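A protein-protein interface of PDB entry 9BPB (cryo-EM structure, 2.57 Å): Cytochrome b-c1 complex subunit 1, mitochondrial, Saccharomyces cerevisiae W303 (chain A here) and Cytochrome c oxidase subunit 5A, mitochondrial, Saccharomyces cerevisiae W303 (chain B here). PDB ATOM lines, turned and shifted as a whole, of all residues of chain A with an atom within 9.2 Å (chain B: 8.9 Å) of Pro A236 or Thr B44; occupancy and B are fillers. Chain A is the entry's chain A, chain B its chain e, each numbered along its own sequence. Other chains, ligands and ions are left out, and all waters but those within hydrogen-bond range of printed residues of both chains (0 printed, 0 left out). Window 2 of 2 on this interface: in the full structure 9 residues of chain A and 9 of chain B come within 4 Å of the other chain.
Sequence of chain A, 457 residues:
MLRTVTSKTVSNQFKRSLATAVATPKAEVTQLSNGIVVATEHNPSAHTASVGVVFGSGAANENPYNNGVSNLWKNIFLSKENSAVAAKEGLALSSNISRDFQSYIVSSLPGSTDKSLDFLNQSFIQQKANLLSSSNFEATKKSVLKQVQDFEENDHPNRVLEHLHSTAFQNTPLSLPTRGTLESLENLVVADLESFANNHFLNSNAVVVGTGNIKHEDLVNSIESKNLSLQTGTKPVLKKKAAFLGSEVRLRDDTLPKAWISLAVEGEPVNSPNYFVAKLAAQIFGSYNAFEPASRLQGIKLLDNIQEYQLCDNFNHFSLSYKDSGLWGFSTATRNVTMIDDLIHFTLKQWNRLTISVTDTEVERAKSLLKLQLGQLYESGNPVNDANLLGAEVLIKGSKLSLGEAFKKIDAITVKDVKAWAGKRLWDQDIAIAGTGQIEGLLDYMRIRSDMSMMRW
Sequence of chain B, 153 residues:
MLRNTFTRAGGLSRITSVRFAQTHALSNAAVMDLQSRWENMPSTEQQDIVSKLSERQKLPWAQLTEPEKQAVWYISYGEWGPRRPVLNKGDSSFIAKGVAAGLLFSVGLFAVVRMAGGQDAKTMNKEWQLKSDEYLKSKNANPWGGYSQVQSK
Among the printed residues, merely in contact across the chains: Asn A199 with Asp B48, Pro A236 with Pro B42, Pro A236 with Thr B44, Val A237 with Pro B42 and Lys A239 with Met B41.
Printed residues of chain B that touch a printed residue of chain A: Met B41, Pro B42, Thr B44 and Asp B48. Hydrophobic or aromatic side chains of chain A within 4 Å of the printed part of chain B: Pro A236. Among the printed residues, 5 pairs touch across the chains.
Pro A236 touches just these residues of chain B: Pro B42 and Thr B44. Of chain A, only Pro A236 (3.3 Å) comes within 4 Å of Thr B44. No residue of chain A comes within 4 Å of Ser B43. No residue of chain A comes within 4 Å of Gln B47. Printed residues of chain A within 4 Å of Met B41: Lys A239 (3.4 Å). Of the printed residues of chain B, Asn A199 touches Asp B48 (3.8 Å). Printed residues of chain A within 4 Å of Asp B48: Asn A199. Of the printed residues of chain B, Lys A239 touches Met B41 (3.4 Å). Gly A56 touches none of the printed residues of chain B. The nearest residue of chain B that does not touch Pro A236 is Glu B45 (4.7 Å). The nearest residue of chain A that does not touch Thr B44 is Lys A235 (4.5 Å).
The backbone carbonyl oxygen of Ser A195 lies close to the side-chain amide oxygen of Asn A199, 2.8 Å away. OE1 of Gln B46 lies close to O of Met B41 (3.4 Å).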
ATOM      1  N   GLY A  56      15.824  26.731 -17.653  1.00  0.00           N
ATOM      2  CA  GLY A  56      16.469  25.711 -16.848  1.00  0.00           C
ATOM      3  C   GLY A  56      17.710  26.189 -16.129  1.00  0.00           C
ATOM      4  O   GLY A  56      18.431  25.375 -15.547  1.00  0.00           O
ATOM      5  N   SER A  57      17.987  27.487 -16.175  1.00  0.00           N
ATOM      6  CA  SER A  57      19.089  28.047 -15.407  1.00  0.00           C
ATOM      7  C   SER A  57      18.557  28.728 -14.152  1.00  0.00           C
ATOM      8  O   SER A  57      17.431  29.225 -14.120  1.00  0.00           O
ATOM      9  CB  SER A  57      19.875  29.045 -16.254  1.00  0.00           C
ATOM     10  OG  SER A  57      20.467  28.405 -17.367  1.00  0.00           O
ATOM     11  N   ALA A  60      22.161  28.552  -9.397  1.00  0.00           N
ATOM     12  CA  ALA A  60      23.275  27.611  -9.384  1.00  0.00           C
ATOM     13  C   ALA A  60      24.116  27.735 -10.649  1.00  0.00           C
ATOM     14  O   ALA A  60      25.189  27.130 -10.752  1.00  0.00           O
ATOM     15  CB  ALA A  60      22.755  26.186  -9.219  1.00  0.00           C
ATOM     16  N   ASN A  61      23.643  28.510 -11.625  1.00  0.00           N
ATOM     17  CA  ASN A  61      24.380  28.648 -12.876  1.00  0.00           C
ATOM     18  C   ASN A  61      25.319  29.847 -12.842  1.00  0.00           C
ATOM     19  O   ASN A  61      26.071  30.081 -13.795  1.00  0.00           O
ATOM     20  CB  ASN A  61      23.410  28.767 -14.048  1.00  0.00           C
ATOM     21  CG  ASN A  61      22.589  27.513 -14.250  1.00  0.00           C
ATOM     22  OD1 ASN A  61      21.679  27.222 -13.477  1.00  0.00           O
ATOM     23  ND2 ASN A  61      22.914  26.755 -15.287  1.00  0.00           N
ATOM     24  N   GLU A  62      25.289  30.622 -11.762  1.00  0.00           N
ATOM     25  CA  GLU A  62      26.172  31.770 -11.653  1.00  0.00           C
ATOM     26  C   GLU A  62      27.293  31.501 -10.649  1.00  0.00           C
ATOM     27  O   GLU A  62      27.283  30.510  -9.916  1.00  0.00           O
ATOM     28  CB  GLU A  62      25.372  33.014 -11.273  1.00  0.00           C
ATOM     29  CG  GLU A  62      24.788  33.002  -9.881  1.00  0.00           C
ATOM     30  CD  GLU A  62      23.544  33.857  -9.787  1.00  0.00           C
ATOM     31  OE1 GLU A  62      23.043  34.285 -10.843  1.00  0.00           O
ATOM     32  OE2 GLU A  62      23.068  34.108  -8.661  1.00  0.00           O
ATOM     33  N   SER A 195      25.925  39.367 -20.890  1.00  0.00           N
ATOM     34  CA  SER A 195      26.664  38.117 -21.022  1.00  0.00           C
ATOM     35  C   SER A 195      25.845  36.938 -20.514  1.00  0.00           C
ATOM     36  O   SER A 195      25.778  35.890 -21.169  1.00  0.00           O
ATOM     37  CB  SER A 195      27.988  38.214 -20.269  1.00  0.00           C
ATOM     38  OG  SER A 195      28.618  36.950 -20.179  1.00  0.00           O
ATOM     39  N   PHE A 196      25.210  37.092 -19.351  1.00  0.00           N
ATOM     40  CA  PHE A 196      24.387  36.011 -18.816  1.00  0.00           C
ATOM     41  C   PHE A 196      23.212  35.709 -19.739  1.00  0.00           C
ATOM     42  O   PHE A 196      22.865  34.541 -19.960  1.00  0.00           O
ATOM     43  CB  PHE A 196      23.893  36.372 -17.417  1.00  0.00           C
ATOM     44  CG  PHE A 196      23.247  35.229 -16.689  1.00  0.00           C
ATOM     45  CD1 PHE A 196      24.012  34.323 -15.980  1.00  0.00           C
ATOM     46  CD2 PHE A 196      21.874  35.059 -16.719  1.00  0.00           C
ATOM     47  CE1 PHE A 196      23.422  33.273 -15.311  1.00  0.00           C
ATOM     48  CE2 PHE A 196      21.279  34.008 -16.057  1.00  0.00           C
ATOM     49  CZ  PHE A 196      22.055  33.116 -15.352  1.00  0.00           C
ATOM     50  N   ALA A 197      22.589  36.752 -20.291  1.00  0.00           N
ATOM     51  CA  ALA A 197      21.484  36.546 -21.221  1.00  0.00           C
ATOM     52  C   ALA A 197      21.945  35.810 -22.473  1.00  0.00           C
ATOM     53  O   ALA A 197      21.227  34.950 -22.995  1.00  0.00           O
ATOM     54  CB  ALA A 197      20.848  37.885 -21.590  1.00  0.00           C
ATOM     55  N   ASN A 198      23.135  36.143 -22.979  1.00  0.00           N
ATOM     56  CA  ASN A 198      23.669  35.433 -24.136  1.00  0.00           C
ATOM     57  C   ASN A 198      23.951  33.975 -23.808  1.00  0.00           C
ATOM     58  O   ASN A 198      23.762  33.093 -24.653  1.00  0.00           O
ATOM     59  CB  ASN A 198      24.944  36.111 -24.639  1.00  0.00           C
ATOM     60  CG  ASN A 198      24.710  37.535 -25.081  1.00  0.00           C
ATOM     61  OD1 ASN A 198      23.580  38.017 -25.088  1.00  0.00           O
ATOM     62  ND2 ASN A 198      25.783  38.220 -25.458  1.00  0.00           N
ATOM     63  N   ASN A 199      24.417  33.700 -22.591  1.00  0.00           N
ATOM     64  CA  ASN A 199      24.869  32.349 -22.284  1.00  0.00           C
ATOM     65  C   ASN A 199      23.720  31.423 -21.903  1.00  0.00           C
ATOM     66  O   ASN A 199      23.830  30.203 -22.072  1.00  0.00           O
ATOM     67  CB  ASN A 199      25.916  32.381 -21.171  1.00  0.00           C
ATOM     68  CG  ASN A 199      27.240  32.945 -21.634  1.00  0.00           C
ATOM     69  OD1 ASN A 199      27.776  33.875 -21.035  1.00  0.00           O
ATOM     70  ND2 ASN A 199      27.777  32.385 -22.710  1.00  0.00           N
ATOM     71  N   HIS A 200      22.614  31.957 -21.376  1.00  0.00           N
ATOM     72  CA  HIS A 200      21.625  31.079 -20.758  1.00  0.00           C
ATOM     73  C   HIS A 200      20.210  31.170 -21.318  1.00  0.00           C
ATOM     74  O   HIS A 200      19.430  30.235 -21.108  1.00  0.00           O
ATOM     75  CB  HIS A 200      21.576  31.328 -19.246  1.00  0.00           C
ATOM     76  CG  HIS A 200      22.811  30.890 -18.527  1.00  0.00           C
ATOM     77  ND1 HIS A 200      22.938  29.640 -17.964  1.00  0.00           N
ATOM     78  CD2 HIS A 200      23.972  31.536 -18.272  1.00  0.00           C
ATOM     79  CE1 HIS A 200      24.124  29.533 -17.396  1.00  0.00           C
ATOM     80  NE2 HIS A 200      24.772  30.670 -17.569  1.00  0.00           N
ATOM     81  N   PHE A 201      19.842  32.240 -22.009  1.00  0.00           N
ATOM     82  CA  PHE A 201      18.477  32.396 -22.517  1.00  0.00           C
ATOM     83  C   PHE A 201      18.419  31.779 -23.912  1.00  0.00           C
ATOM     84  O   PHE A 201      18.551  32.478 -24.919  1.00  0.00           O
ATOM     85  CB  PHE A 201      18.058  33.863 -22.526  1.00  0.00           C
ATOM     86  CG  PHE A 201      17.873  34.454 -21.153  1.00  0.00           C
ATOM     87  CD1 PHE A 201      17.953  33.661 -20.019  1.00  0.00           C
ATOM     88  CD2 PHE A 201      17.613  35.805 -20.996  1.00  0.00           C
ATOM     89  CE1 PHE A 201      17.783  34.202 -18.760  1.00  0.00           C
ATOM     90  CE2 PHE A 201      17.442  36.349 -19.738  1.00  0.00           C
ATOM     91  CZ  PHE A 201      17.528  35.547 -18.622  1.00  0.00           C
ATOM     92  N   LEU A 202      18.198  30.466 -23.966  1.00  0.00           N
ATOM     93  CA  LEU A 202      18.375  29.696 -25.189  1.00  0.00           C
ATOM     94  C   LEU A 202      17.135  28.854 -25.462  1.00  0.00           C
ATOM     95  O   LEU A 202      16.350  28.561 -24.559  1.00  0.00           O
ATOM     96  CB  LEU A 202      19.609  28.792 -25.090  1.00  0.00           C
ATOM     97  CG  LEU A 202      20.927  29.513 -24.806  1.00  0.00           C
ATOM     98  CD1 LEU A 202      22.021  28.514 -24.535  1.00  0.00           C
ATOM     99  CD2 LEU A 202      21.312  30.419 -25.954  1.00  0.00           C
ATOM    100  N   SER A 204      17.103  25.686 -26.289  1.00  0.00           N
ATOM    101  CA  SER A 204      17.212  24.329 -25.766  1.00  0.00           C
ATOM    102  C   SER A 204      17.064  24.299 -24.251  1.00  0.00           C
ATOM    103  O   SER A 204      17.023  23.223 -23.644  1.00  0.00           O
ATOM    104  CB  SER A 204      18.542  23.710 -26.189  1.00  0.00           C
ATOM    105  OG  SER A 204      19.630  24.504 -25.757  1.00  0.00           O
ATOM    106  N   ASN A 205      16.995  25.468 -23.620  1.00  0.00           N
ATOM    107  CA  ASN A 205      16.911  25.575 -22.171  1.00  0.00           C
ATOM    108  C   ASN A 205      15.543  26.031 -21.677  1.00  0.00           C
ATOM    109  O   ASN A 205      15.364  26.201 -20.469  1.00  0.00           O
ATOM    110  CB  ASN A 205      17.980  26.542 -21.662  1.00  0.00           C
ATOM    111  CG  ASN A 205      18.463  26.200 -20.277  1.00  0.00           C
ATOM    112  OD1 ASN A 205      18.158  25.135 -19.750  1.00  0.00           O
ATOM    113  ND2 ASN A 205      19.213  27.108 -19.673  1.00  0.00           N
ATOM    114  N   GLY A 233      21.585  27.832 -28.849  1.00  0.00           N
ATOM    115  CA  GLY A 233      21.667  26.747 -27.898  1.00  0.00           C
ATOM    116  C   GLY A 233      23.063  26.630 -27.328  1.00  0.00           C
ATOM    117  O   GLY A 233      23.845  27.578 -27.372  1.00  0.00           O
ATOM    118  N   THR A 234      23.359  25.442 -26.796  1.00  0.00           N
ATOM    119  CA  THR A 234      24.658  25.126 -26.190  1.00  0.00           C
ATOM    120  C   THR A 234      24.973  26.042 -25.006  1.00  0.00           C
ATOM    121  O   THR A 234      25.899  26.853 -25.044  1.00  0.00           O
ATOM    122  CB  THR A 234      25.782  25.173 -27.229  1.00  0.00           C
ATOM    123  OG1 THR A 234      26.032  26.531 -27.617  1.00  0.00           O
ATOM    124  CG2 THR A 234      25.413  24.353 -28.459  1.00  0.00           C
ATOM    125  N   LYS A 235      24.178  25.913 -23.944  1.00  0.00           N
ATOM    126  CA  LYS A 235      24.476  26.607 -22.702  1.00  0.00           C
ATOM    127  C   LYS A 235      25.724  26.006 -22.054  1.00  0.00           C
ATOM    128  O   LYS A 235      26.060  24.844 -22.302  1.00  0.00           O
ATOM    129  CB  LYS A 235      23.288  26.520 -21.744  1.00  0.00           C
ATOM    130  CG  LYS A 235      22.964  25.110 -21.290  1.00  0.00           C
ATOM    131  CD  LYS A 235      21.794  25.089 -20.323  1.00  0.00           C
ATOM    132  CE  LYS A 235      22.175  25.628 -18.961  1.00  0.00           C
ATOM    133  NZ  LYS A 235      23.120  24.717 -18.268  1.00  0.00           N
ATOM    134  N   PRO A 236      26.436  26.778 -21.232  1.00  0.00           N
ATOM    135  CA  PRO A 236      27.629  26.237 -20.568  1.00  0.00           C
ATOM    136  C   PRO A 236      27.280  25.058 -19.673  1.00  0.00           C
ATOM    137  O   PRO A 236      26.222  25.022 -19.043  1.00  0.00           O
ATOM    138  CB  PRO A 236      28.148  27.427 -19.752  1.00  0.00           C
ATOM    139  CG  PRO A 236      27.580  28.623 -20.423  1.00  0.00           C
ATOM    140  CD  PRO A 236      26.238  28.203 -20.924  1.00  0.00           C
ATOM    141  N   VAL A 237      28.186  24.087 -19.623  1.00  0.00           N
ATOM    142  CA  VAL A 237      28.042  22.914 -18.772  1.00  0.00           C
ATOM    143  C   VAL A 237      28.953  23.085 -17.564  1.00  0.00           C
ATOM    144  O   VAL A 237      30.127  23.447 -17.707  1.00  0.00           O
ATOM    145  CB  VAL A 237      28.346  21.613 -19.538  1.00  0.00           C
ATOM    146  CG1 VAL A 237      27.350  21.426 -20.666  1.00  0.00           C
ATOM    147  CG2 VAL A 237      29.755  21.627 -20.101  1.00  0.00           C
ATOM    148  N   LEU A 238      28.402  22.860 -16.376  1.00  0.00           N
ATOM    149  CA  LEU A 238      29.164  23.046 -15.150  1.00  0.00           C
ATOM    150  C   LEU A 238      30.205  21.944 -15.001  1.00  0.00           C
ATOM    151  O   LEU A 238      29.942  20.779 -15.315  1.00  0.00           O
ATOM    152  CB  LEU A 238      28.230  23.062 -13.944  1.00  0.00           C
ATOM    153  CG  LEU A 238      27.226  24.215 -13.892  1.00  0.00           C
ATOM    154  CD1 LEU A 238      26.360  24.106 -12.651  1.00  0.00           C
ATOM    155  CD2 LEU A 238      27.939  25.557 -13.937  1.00  0.00           C
ATOM    156  N   LYS A 239      31.392  22.304 -14.514  1.00  0.00           N
ATOM    157  CA  LYS A 239      32.501  21.325 -14.378  1.00  0.00           C
ATOM    158  C   LYS A 239      32.385  20.552 -13.064  1.00  0.00           C
ATOM    159  O   LYS A 239      32.896  19.427 -13.008  1.00  0.00           O
ATOM    160  CB  LYS A 239      33.855  22.033 -14.453  1.00  0.00           C
ATOM    161  CG  LYS A 239      34.282  22.481 -15.843  1.00  0.00           C
ATOM    162  CD  LYS A 239      35.717  22.947 -15.889  1.00  0.00           C
ATOM    163  CE  LYS A 239      36.267  23.037 -17.295  1.00  0.00           C
ATOM    164  NZ  LYS A 239      37.668  23.522 -17.298  1.00  0.00           N
ATOM    165  N   MET B  41      35.723  26.383 -14.496  1.00  0.00           N
ATOM    166  CA  MET B  41      35.049  27.438 -15.311  1.00  0.00           C
ATOM    167  C   MET B  41      34.544  26.857 -16.642  1.00  0.00           C
ATOM    168  O   MET B  41      35.375  26.313 -17.379  1.00  0.00           O
ATOM    169  CB  MET B  41      36.068  28.543 -15.599  1.00  0.00           C
ATOM    170  CG  MET B  41      35.683  29.540 -16.661  1.00  0.00           C
ATOM    171  SD  MET B  41      36.936  30.847 -16.704  1.00  0.00           S
ATOM    172  CE  MET B  41      35.959  32.229 -17.289  1.00  0.00           C
ATOM    173  N   PRO B  42      33.240  26.973 -17.005  1.00  0.00           N
ATOM    174  CA  PRO B  42      32.692  26.329 -18.207  1.00  0.00           C
ATOM    175  C   PRO B  42      33.539  26.620 -19.438  1.00  0.00           C
ATOM    176  O   PRO B  42      34.057  27.725 -19.614  1.00  0.00           O
ATOM    177  CB  PRO B  42      31.293  26.940 -18.326  1.00  0.00           C
ATOM    178  CG  PRO B  42      30.938  27.318 -16.927  1.00  0.00           C
ATOM    179  CD  PRO B  42      32.224  27.771 -16.298  1.00  0.00           C
ATOM    180  N   SER B  43      33.679  25.601 -20.290  1.00  0.00           N
ATOM    181  CA  SER B  43      34.541  25.723 -21.463  1.00  0.00           C
ATOM    182  C   SER B  43      34.020  26.777 -22.432  1.00  0.00           C
ATOM    183  O   SER B  43      34.797  27.576 -22.966  1.00  0.00           O
ATOM    184  CB  SER B  43      34.668  24.371 -22.160  1.00  0.00           C
ATOM    185  OG  SER B  43      35.092  24.531 -23.503  1.00  0.00           O
ATOM    186  N   THR B  44      32.708  26.791 -22.677  1.00  0.00           N
ATOM    187  CA  THR B  44      32.139  27.814 -23.549  1.00  0.00           C
ATOM    188  C   THR B  44      32.234  29.193 -22.909  1.00  0.00           C
ATOM    189  O   THR B  44      32.406  30.199 -23.610  1.00  0.00           O
ATOM    190  CB  THR B  44      30.685  27.476 -23.883  1.00  0.00           C
ATOM    191  OG1 THR B  44      29.933  27.339 -22.671  1.00  0.00           O
ATOM    192  CG2 THR B  44      30.608  26.179 -24.673  1.00  0.00           C
ATOM    193  N   GLU B  45      32.117  29.261 -21.581  1.00  0.00           N
ATOM    194  CA  GLU B  45      32.241  30.538 -20.888  1.00  0.00           C
ATOM    195  C   GLU B  45      33.660  31.087 -20.992  1.00  0.00           C
ATOM    196  O   GLU B  45      33.851  32.298 -21.157  1.00  0.00           O
ATOM    197  CB  GLU B  45      31.825  30.378 -19.425  1.00  0.00           C
ATOM    198  CG  GLU B  45      32.211  31.541 -18.530  1.00  0.00           C
ATOM    199  CD  GLU B  45      31.352  31.629 -17.285  1.00  0.00           C
ATOM    200  OE1 GLU B  45      30.365  30.869 -17.188  1.00  0.00           O
ATOM    201  OE2 GLU B  45      31.664  32.456 -16.403  1.00  0.00           O
ATOM    202  N   GLN B  46      34.666  30.214 -20.902  1.00  0.00           N
ATOM    203  CA  GLN B  46      36.051  30.662 -20.964  1.00  0.00           C
ATOM    204  C   GLN B  46      36.546  30.866 -22.389  1.00  0.00           C
ATOM    205  O   GLN B  46      37.619  31.449 -22.577  1.00  0.00           O
ATOM    206  CB  GLN B  46      36.964  29.672 -20.237  1.00  0.00           C
ATOM    207  CG  GLN B  46      37.414  28.490 -21.077  1.00  0.00           C
ATOM    208  CD  GLN B  46      38.040  27.393 -20.244  1.00  0.00           C
ATOM    209  OE1 GLN B  46      38.071  27.472 -19.019  1.00  0.00           O
ATOM    210  NE2 GLN B  46      38.546  26.361 -20.908  1.00  0.00           N
ATOM    211  N   GLN B  47      35.809  30.394 -23.395  1.00  0.00           N
ATOM    212  CA  GLN B  47      36.191  30.681 -24.773  1.00  0.00           C
ATOM    213  C   GLN B  47      35.669  32.030 -25.247  1.00  0.00           C
ATOM    214  O   GLN B  47      36.136  32.533 -26.275  1.00  0.00           O
ATOM    215  CB  GLN B  47      35.698  29.572 -25.706  1.00  0.00           C
ATOM    216  CG  GLN B  47      34.313  29.797 -26.285  1.00  0.00           C
ATOM    217  CD  GLN B  47      33.810  28.600 -27.070  1.00  0.00           C
ATOM    218  OE1 GLN B  47      34.538  27.630 -27.278  1.00  0.00           O
ATOM    219  NE2 GLN B  47      32.559  28.665 -27.510  1.00  0.00           N
ATOM    220  N   ASP B  48      34.714  32.623 -24.526  1.00  0.00           N
ATOM    221  CA  ASP B  48      34.268  33.976 -24.836  1.00  0.00           C
ATOM    222  C   ASP B  48      35.248  35.029 -24.335  1.00  0.00           C
ATOM    223  O   ASP B  48      35.372  36.093 -24.950  1.00  0.00           O
ATOM    224  CB  ASP B  48      32.886  34.232 -24.234  1.00  0.00           C
ATOM    225  CG  ASP B  48      31.761  33.761 -25.132  1.00  0.00           C
ATOM    226  OD1 ASP B  48      32.055  33.221 -26.221  1.00  0.00           O
ATOM    227  OD2 ASP B  48      30.585  33.933 -24.753  1.00  0.00           O
ATOM    228  N   ILE B  49      35.941  34.758 -23.227  1.00  0.00           N
ATOM    229  CA  ILE B  49      36.846  35.751 -22.657  1.00  0.00           C
ATOM    230  C   ILE B  49      38.053  35.969 -23.566  1.00  0.00           C
ATOM    231  O   ILE B  49      38.542  37.096 -23.706  1.00  0.00           O
ATOM    232  CB  ILE B  49      37.259  35.349 -21.225  1.00  0.00           C
ATOM    233  CG1 ILE B  49      37.856  36.540 -20.478  1.00  0.00           C
ATOM    234  CG2 ILE B  49      38.240  34.190 -21.224  1.00  0.00           C
ATOM    235  CD1 ILE B  49      36.855  37.622 -20.157  1.00  0.00           C
ATOM    236  N   VAL B  50      38.543  34.906 -24.212  1.00  0.00           N
ATOM    237  CA  VAL B  50      39.737  35.043 -25.043  1.00  0.00           C
ATOM    238  C   VAL B  50      39.410  35.747 -26.352  1.00  0.00           C
ATOM    239  O   VAL B  50      40.289  36.361 -26.969  1.00  0.00           O
ATOM    240  CB  VAL B  50      40.392  33.671 -25.289  1.00  0.00           C
ATOM    241  CG1 VAL B  50      40.699  32.983 -23.970  1.00  0.00           C
ATOM    242  CG2 VAL B  50      39.504  32.797 -26.157  1.00  0.00           C
ATOM    243  N   SER B  51      38.157  35.667 -26.807  1.00  0.00           N
ATOM    244  CA  SER B  51      37.760  36.422 -27.989  1.00  0.00           C
ATOM    245  C   SER B  51      37.730  37.918 -27.699  1.00  0.00           C
ATOM    246  O   SER B  51      38.138  38.728 -28.538  1.00  0.00           O
ATOM    247  CB  SER B  51      36.399  35.941 -28.490  1.00  0.00           C
ATOM    248  OG  SER B  51      35.942  36.735 -29.571  1.00  0.00           O
